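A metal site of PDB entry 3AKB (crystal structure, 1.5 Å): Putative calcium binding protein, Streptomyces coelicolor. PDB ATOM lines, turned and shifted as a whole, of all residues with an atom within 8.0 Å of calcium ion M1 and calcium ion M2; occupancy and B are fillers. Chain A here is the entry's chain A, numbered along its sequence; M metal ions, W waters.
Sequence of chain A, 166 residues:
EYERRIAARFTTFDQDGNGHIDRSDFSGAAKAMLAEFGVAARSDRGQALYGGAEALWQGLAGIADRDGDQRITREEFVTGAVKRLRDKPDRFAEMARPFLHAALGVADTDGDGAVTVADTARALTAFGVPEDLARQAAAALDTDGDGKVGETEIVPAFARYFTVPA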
ATOM      1  N   PHE A  10      -6.681 -26.009 -26.752  1.00  0.00           N
ATOM      2  CA  PHE A  10      -5.251 -25.752 -26.793  1.00  0.00           C
ATOM      3  C   PHE A  10      -4.800 -24.817 -25.675  1.00  0.00           C
ATOM      4  O   PHE A  10      -3.795 -25.070 -25.005  1.00  0.00           O
ATOM      5  CB  PHE A  10      -4.811 -25.191 -28.153  1.00  0.00           C
ATOM      6  CG  PHE A  10      -3.318 -25.025 -28.289  1.00  0.00           C
ATOM      7  CD1 PHE A  10      -2.523 -26.129 -28.570  1.00  0.00           C
ATOM      8  CD2 PHE A  10      -2.728 -23.792 -28.119  1.00  0.00           C
ATOM      9  CE1 PHE A  10      -1.127 -25.989 -28.667  1.00  0.00           C
ATOM     10  CE2 PHE A  10      -1.326 -23.651 -28.223  1.00  0.00           C
ATOM     11  CZ  PHE A  10      -0.543 -24.762 -28.503  1.00  0.00           C
ATOM     12  N   THR A  11      -5.529 -23.708 -25.499  1.00  0.00           N
ATOM     13  CA  THR A  11      -5.234 -22.726 -24.466  1.00  0.00           C
ATOM     14  C   THR A  11      -5.252 -23.337 -23.062  1.00  0.00           C
ATOM     15  O   THR A  11      -4.427 -22.968 -22.215  1.00  0.00           O
ATOM     16  CB  THR A  11      -6.233 -21.535 -24.548  1.00  0.00           C
ATOM     17  OG1 THR A  11      -6.141 -20.908 -25.840  1.00  0.00           O
ATOM     18  CG2 THR A  11      -5.958 -20.488 -23.479  1.00  0.00           C
ATOM     19  N   PHE A  13      -4.361 -26.280 -22.245  1.00  0.00           N
ATOM     20  CA  PHE A  13      -3.078 -26.994 -22.048  1.00  0.00           C
ATOM     21  C   PHE A  13      -1.882 -26.042 -22.043  1.00  0.00           C
ATOM     22  O   PHE A  13      -0.914 -26.236 -21.301  1.00  0.00           O
ATOM     23  CB  PHE A  13      -2.872 -28.042 -23.147  1.00  0.00           C
ATOM     24  CG  PHE A  13      -3.736 -29.285 -23.010  1.00  0.00           C
ATOM     25  CD1 PHE A  13      -3.794 -29.995 -21.812  1.00  0.00           C
ATOM     26  CD2 PHE A  13      -4.422 -29.776 -24.126  1.00  0.00           C
ATOM     27  CE1 PHE A  13      -4.592 -31.187 -21.727  1.00  0.00           C
ATOM     28  CE2 PHE A  13      -5.209 -30.957 -24.057  1.00  0.00           C
ATOM     29  CZ  PHE A  13      -5.287 -31.661 -22.850  1.00  0.00           C
ATOM     30  N   ASP A  14      -1.961 -24.999 -22.877  1.00  0.00           N
ATOM     31  CA  ASP A  14      -0.874 -24.015 -22.998  1.00  0.00           C
ATOM     32  C   ASP A  14      -1.007 -22.985 -21.896  1.00  0.00           C
ATOM     33  O   ASP A  14      -1.273 -21.802 -22.126  1.00  0.00           O
ATOM     34  CB  ASP A  14      -0.899 -23.370 -24.382  1.00  0.00           C
ATOM     35  CG  ASP A  14       0.244 -22.405 -24.594  1.00  0.00           C
ATOM     36  OD1 ASP A  14       1.287 -22.564 -23.897  1.00  0.00           O
ATOM     37  OD2 ASP A  14       0.117 -21.485 -25.453  1.00  0.00           O
ATOM     38  N   GLN A  15      -0.732 -23.448 -20.671  1.00  0.00           N
ATOM     39  CA  GLN A  15      -0.934 -22.669 -19.464  1.00  0.00           C
ATOM     40  C   GLN A  15      -0.154 -21.364 -19.432  1.00  0.00           C
ATOM     41  O   GLN A  15      -0.666 -20.367 -18.913  1.00  0.00           O
ATOM     42  CB  GLN A  15      -0.639 -23.537 -18.242  1.00  0.00           C
ATOM     43  CG  GLN A  15      -1.747 -24.562 -17.960  1.00  0.00           C
ATOM     44  CD  GLN A  15      -2.951 -23.940 -17.269  1.00  0.00           C
ATOM     45  OE1 GLN A  15      -2.793 -23.243 -16.266  1.00  0.00           O
ATOM     46  NE2 GLN A  15      -4.150 -24.209 -17.762  1.00  0.00           N
ATOM     47  N   ASP A  16       1.064 -21.340 -20.001  1.00  0.00           N
ATOM     48  CA  ASP A  16       1.857 -20.106 -20.010  1.00  0.00           C
ATOM     49  C   ASP A  16       1.645 -19.229 -21.260  1.00  0.00           C
ATOM     50  O   ASP A  16       2.224 -18.141 -21.389  1.00  0.00           O
ATOM     51  CB  ASP A  16       3.347 -20.413 -19.730  1.00  0.00           C
ATOM     52  CG  ASP A  16       4.035 -21.134 -20.867  1.00  0.00           C
ATOM     53  OD1 ASP A  16       3.504 -21.215 -21.999  1.00  0.00           O
ATOM     54  OD2 ASP A  16       5.174 -21.595 -20.604  1.00  0.00           O
ATOM     55  N   GLY A  17       0.784 -19.696 -22.147  1.00  0.00           N
ATOM     56  CA  GLY A  17       0.322 -18.901 -23.294  1.00  0.00           C
ATOM     57  C   GLY A  17       1.299 -18.688 -24.424  1.00  0.00           C
ATOM     58  O   GLY A  17       1.057 -17.853 -25.302  1.00  0.00           O
ATOM     59  N   ASN A  18       2.404 -19.444 -24.436  1.00  0.00           N
ATOM     60  CA  ASN A  18       3.477 -19.132 -25.373  1.00  0.00           C
ATOM     61  C   ASN A  18       3.391 -19.879 -26.732  1.00  0.00           C
ATOM     62  O   ASN A  18       4.322 -19.831 -27.556  1.00  0.00           O
ATOM     63  CB  ASN A  18       4.817 -19.346 -24.679  1.00  0.00           C
ATOM     64  CG  ASN A  18       5.148 -20.815 -24.516  1.00  0.00           C
ATOM     65  OD1 ASN A  18       4.345 -21.707 -24.782  1.00  0.00           O
ATOM     66  ND2 ASN A  18       6.380 -21.070 -24.120  1.00  0.00           N
ATOM     67  N   GLY A  19       2.261 -20.538 -26.969  1.00  0.00           N
ATOM     68  CA  GLY A  19       1.964 -21.119 -28.289  1.00  0.00           C
ATOM     69  C   GLY A  19       2.390 -22.547 -28.532  1.00  0.00           C
ATOM     70  O   GLY A  19       2.136 -23.118 -29.599  1.00  0.00           O
ATOM     71  N   HIS A  20       3.034 -23.153 -27.526  1.00  0.00           N
ATOM     72  CA  HIS A  20       3.310 -24.565 -27.617  1.00  0.00           C
ATOM     73  C   HIS A  20       3.179 -25.160 -26.228  1.00  0.00           C
ATOM     74  O   HIS A  20       3.381 -24.469 -25.239  1.00  0.00           O
ATOM     75  CB  HIS A  20       4.705 -24.837 -28.223  1.00  0.00           C
ATOM     76  CG  HIS A  20       5.862 -24.340 -27.399  1.00  0.00           C
ATOM     77  ND1 HIS A  20       6.527 -23.168 -27.671  1.00  0.00           N
ATOM     78  CD2 HIS A  20       6.501 -24.919 -26.350  1.00  0.00           C
ATOM     79  CE1 HIS A  20       7.506 -23.007 -26.799  1.00  0.00           C
ATOM     80  NE2 HIS A  20       7.531 -24.070 -25.997  1.00  0.00           N
ATOM     81  N   ILE A  21       2.839 -26.438 -26.171  1.00  0.00           N
ATOM     82  CA  ILE A  21       2.643 -27.143 -24.899  1.00  0.00           C
ATOM     83  C   ILE A  21       3.944 -27.883 -24.554  1.00  0.00           C
ATOM     84  O   ILE A  21       4.456 -28.646 -25.386  1.00  0.00           O
ATOM     85  CB  ILE A  21       1.478 -28.129 -24.993  1.00  0.00           C
ATOM     86  CG1 ILE A  21       0.205 -27.386 -25.425  1.00  0.00           C
ATOM     87  CG2 ILE A  21       1.263 -28.808 -23.634  1.00  0.00           C
ATOM     88  CD1 ILE A  21      -0.865 -28.253 -26.057  1.00  0.00           C
ATOM     89  N   ASP A  22       4.460 -27.607 -23.346  1.00  0.00           N
ATOM     90  CA  ASP A  22       5.668 -28.207 -22.754  1.00  0.00           C
ATOM     91  C   ASP A  22       5.315 -28.931 -21.461  1.00  0.00           C
ATOM     92  O   ASP A  22       4.267 -28.660 -20.854  1.00  0.00           O
ATOM     93  CB  ASP A  22       6.648 -27.122 -22.239  1.00  0.00           C
ATOM     94  CG  ASP A  22       7.391 -26.405 -23.311  1.00  0.00           C
ATOM     95  OD1 ASP A  22       7.844 -26.997 -24.324  1.00  0.00           O
ATOM     96  OD2 ASP A  22       7.542 -25.177 -23.093  1.00  0.00           O
ATOM     97  N   ARG A  23       6.230 -29.768 -20.984  1.00  0.00           N
ATOM     98  CA  ARG A  23       6.053 -30.342 -19.655  1.00  0.00           C
ATOM     99  C   ARG A  23       5.887 -29.211 -18.645  1.00  0.00           C
ATOM    100  O   ARG A  23       5.139 -29.351 -17.702  1.00  0.00           O
ATOM    101  CB  ARG A  23       7.219 -31.245 -19.261  1.00  0.00           C
ATOM    102  CG  ARG A  23       6.935 -32.039 -17.994  1.00  0.00           C
ATOM    103  CD  ARG A  23       8.135 -32.840 -17.576  1.00  0.00           C
ATOM    104  NE  ARG A  23       9.114 -31.985 -16.939  1.00  0.00           N
ATOM    105  CZ  ARG A  23      10.151 -32.441 -16.240  1.00  0.00           C
ATOM    106  NH1 ARG A  23      10.356 -33.755 -16.126  1.00  0.00           N
ATOM    107  NH2 ARG A  23      10.979 -31.565 -15.701  1.00  0.00           N
ATOM    108  N   SER A  24       6.582 -28.105 -18.853  1.00  0.00           N
ATOM    109  CA  SER A  24       6.560 -26.991 -17.899  1.00  0.00           C
ATOM    110  C   SER A  24       5.175 -26.338 -17.789  1.00  0.00           C
ATOM    111  O   SER A  24       4.829 -25.762 -16.755  1.00  0.00           O
ATOM    112  CB  SER A  24       7.603 -25.937 -18.201  1.00  0.00           C
ATOM    113  OG  SER A  24       7.396 -25.395 -19.473  1.00  0.00           O
ATOM    114  N   ASP A  25       4.356 -26.433 -18.834  1.00  0.00           N
ATOM    115  CA  ASP A  25       2.978 -25.924 -18.727  1.00  0.00           C
ATOM    116  C   ASP A  25       2.230 -26.693 -17.653  1.00  0.00           C
ATOM    117  O   ASP A  25       1.490 -26.103 -16.843  1.00  0.00           O
ATOM    118  CB  ASP A  25       2.234 -26.085 -20.054  1.00  0.00           C
ATOM    119  CG  ASP A  25       2.583 -25.029 -21.105  1.00  0.00           C
ATOM    120  OD1 ASP A  25       2.460 -23.799 -20.839  1.00  0.00           O
ATOM    121  OD2 ASP A  25       2.962 -25.433 -22.238  1.00  0.00           O
ATOM    122  N   PHE A  26       2.439 -28.005 -17.652  1.00  0.00           N
ATOM    123  CA  PHE A  26       1.788 -28.927 -16.693  1.00  0.00           C
ATOM    124  C   PHE A  26       2.350 -28.783 -15.282  1.00  0.00           C
ATOM    125  O   PHE A  26       1.578 -28.732 -14.317  1.00  0.00           O
ATOM    126  CB  PHE A  26       1.913 -30.366 -17.197  1.00  0.00           C
ATOM    127  CG  PHE A  26       1.000 -30.681 -18.347  1.00  0.00           C
ATOM    128  CD1 PHE A  26      -0.244 -31.282 -18.123  1.00  0.00           C
ATOM    129  CD2 PHE A  26       1.393 -30.414 -19.675  1.00  0.00           C
ATOM    130  CE1 PHE A  26      -1.091 -31.577 -19.171  1.00  0.00           C
ATOM    131  CE2 PHE A  26       0.522 -30.709 -20.719  1.00  0.00           C
ATOM    132  CZ  PHE A  26      -0.720 -31.282 -20.460  1.00  0.00           C
ATOM    133  N   ASP A  69      10.146 -33.642 -30.342  1.00  0.00           N
ATOM    134  CA  ASP A  69      10.958 -32.599 -29.733  1.00  0.00           C
ATOM    135  C   ASP A  69      10.417 -32.165 -28.372  1.00  0.00           C
ATOM    136  O   ASP A  69      10.957 -31.231 -27.775  1.00  0.00           O
ATOM    137  CB  ASP A  69      11.135 -31.399 -30.679  1.00  0.00           C
ATOM    138  CG  ASP A  69       9.861 -30.583 -30.879  1.00  0.00           C
ATOM    139  OD1 ASP A  69       8.741 -31.050 -30.531  1.00  0.00           O
ATOM    140  OD2 ASP A  69       9.992 -29.435 -31.399  1.00  0.00           O
ATOM    141  N   GLN A  70       9.361 -32.830 -27.886  1.00  0.00           N
ATOM    142  CA  GLN A  70       8.820 -32.559 -26.537  1.00  0.00           C
ATOM    143  C   GLN A  70       8.289 -31.133 -26.362  1.00  0.00           C
ATOM    144  O   GLN A  70       8.335 -30.535 -25.275  1.00  0.00           O
ATOM    145  CB  GLN A  70       9.856 -32.993 -25.469  1.00  0.00           C
ATOM    146  CG  GLN A  70      10.097 -34.514 -25.512  1.00  0.00           C
ATOM    147  CD  GLN A  70      11.283 -34.985 -24.673  1.00  0.00           C
ATOM    148  OE1 GLN A  70      12.031 -34.183 -24.113  1.00  0.00           O
ATOM    149  NE2 GLN A  70      11.448 -36.304 -24.601  1.00  0.00           N
ATOM    150  N   ARG A  71       7.813 -30.577 -27.476  1.00  0.00           N
ATOM    151  CA  ARG A  71       6.985 -29.373 -27.551  1.00  0.00           C
ATOM    152  C   ARG A  71       5.812 -29.788 -28.450  1.00  0.00           C
ATOM    153  O   ARG A  71       6.012 -30.449 -29.493  1.00  0.00           O
ATOM    154  CB  ARG A  71       7.719 -28.202 -28.205  1.00  0.00           C
ATOM    155  CG  ARG A  71       8.893 -27.635 -27.409  1.00  0.00           C
ATOM    156  CD  ARG A  71       9.504 -26.432 -28.115  1.00  0.00           C
ATOM    157  NE  ARG A  71      10.232 -26.888 -29.283  1.00  0.00           N
ATOM    158  CZ  ARG A  71      11.545 -27.110 -29.292  1.00  0.00           C
ATOM    159  NH1 ARG A  71      12.240 -26.886 -28.183  1.00  0.00           N
ATOM    160  NH2 ARG A  71      12.135 -27.530 -30.395  1.00  0.00           N
ATOM    161  N   ILE A  72       4.597 -29.443 -28.052  1.00  0.00           N
ATOM    162  CA  ILE A  72       3.440 -29.676 -28.920  1.00  0.00           C
ATOM    163  C   ILE A  72       3.003 -28.332 -29.465  1.00  0.00           C
ATOM    164  O   ILE A  72       2.515 -27.484 -28.726  1.00  0.00           O
ATOM    165  CB  ILE A  72       2.252 -30.290 -28.140  1.00  0.00           C
ATOM    166  CG1 ILE A  72       2.682 -31.615 -27.482  1.00  0.00           C
ATOM    167  CG2 ILE A  72       1.052 -30.492 -29.078  1.00  0.00           C
ATOM    168  CD1 ILE A  72       1.703 -32.121 -26.405  1.00  0.00           C
HETATM  169 CA    CA M   1       3.346 -23.241 -23.223  1.00  0.00          CA
HETATM  170 CA    CA M   2       8.844 -24.295 -24.542  1.00  0.00          CA
HETATM  171  O   HOH W   1       5.557 -23.497 -22.450  1.00  0.00           O
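Calcium ion M2 is bound by NE2 of His 20 (2.0 Å), OD2 of Asp 22 (2.1 Å) and OD1 of Asp 22 (2.9 Å).
Calcium ion M2 has three donor atoms within binding distance.
Water W1 bridges the side-chain carboxylate of Asp 16 (2.7 Å) and the side-chain amide nitrogen of Asn 18 (3.1 Å).
Within 4 Å of calcium ion M2: His 20 and Asp 22.
The nearest printed residue that does not touch calcium ion M2 is Asn 18 (4.1 Å).
Calcium ion M1 is bound by OD1 of Asp 14 (2.3 Å), water W1 (2.4 Å), O of His 20 (2.4 Å), OD1 of Asp 16 (2.4 Å), OD1 of Asn 18 (2.4 Å), OD2 of Asp 25 (2.4 Å) and OD1 of Asp 25 (2.6 Å).
N of Gly 17 sits close to OD1 of Asp 14, at 3.4 Å.
N of Asp 22 lies close to OD2 of Asp 25 (2.9 Å).
The side-chain carboxylate (OD2) of Asp 14 sits at hydrogen-bond distance from the backbone NH (N) of Gly 19.
OD1 of Asp 25 lies close to N of Gln 15 (3.2 Å).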
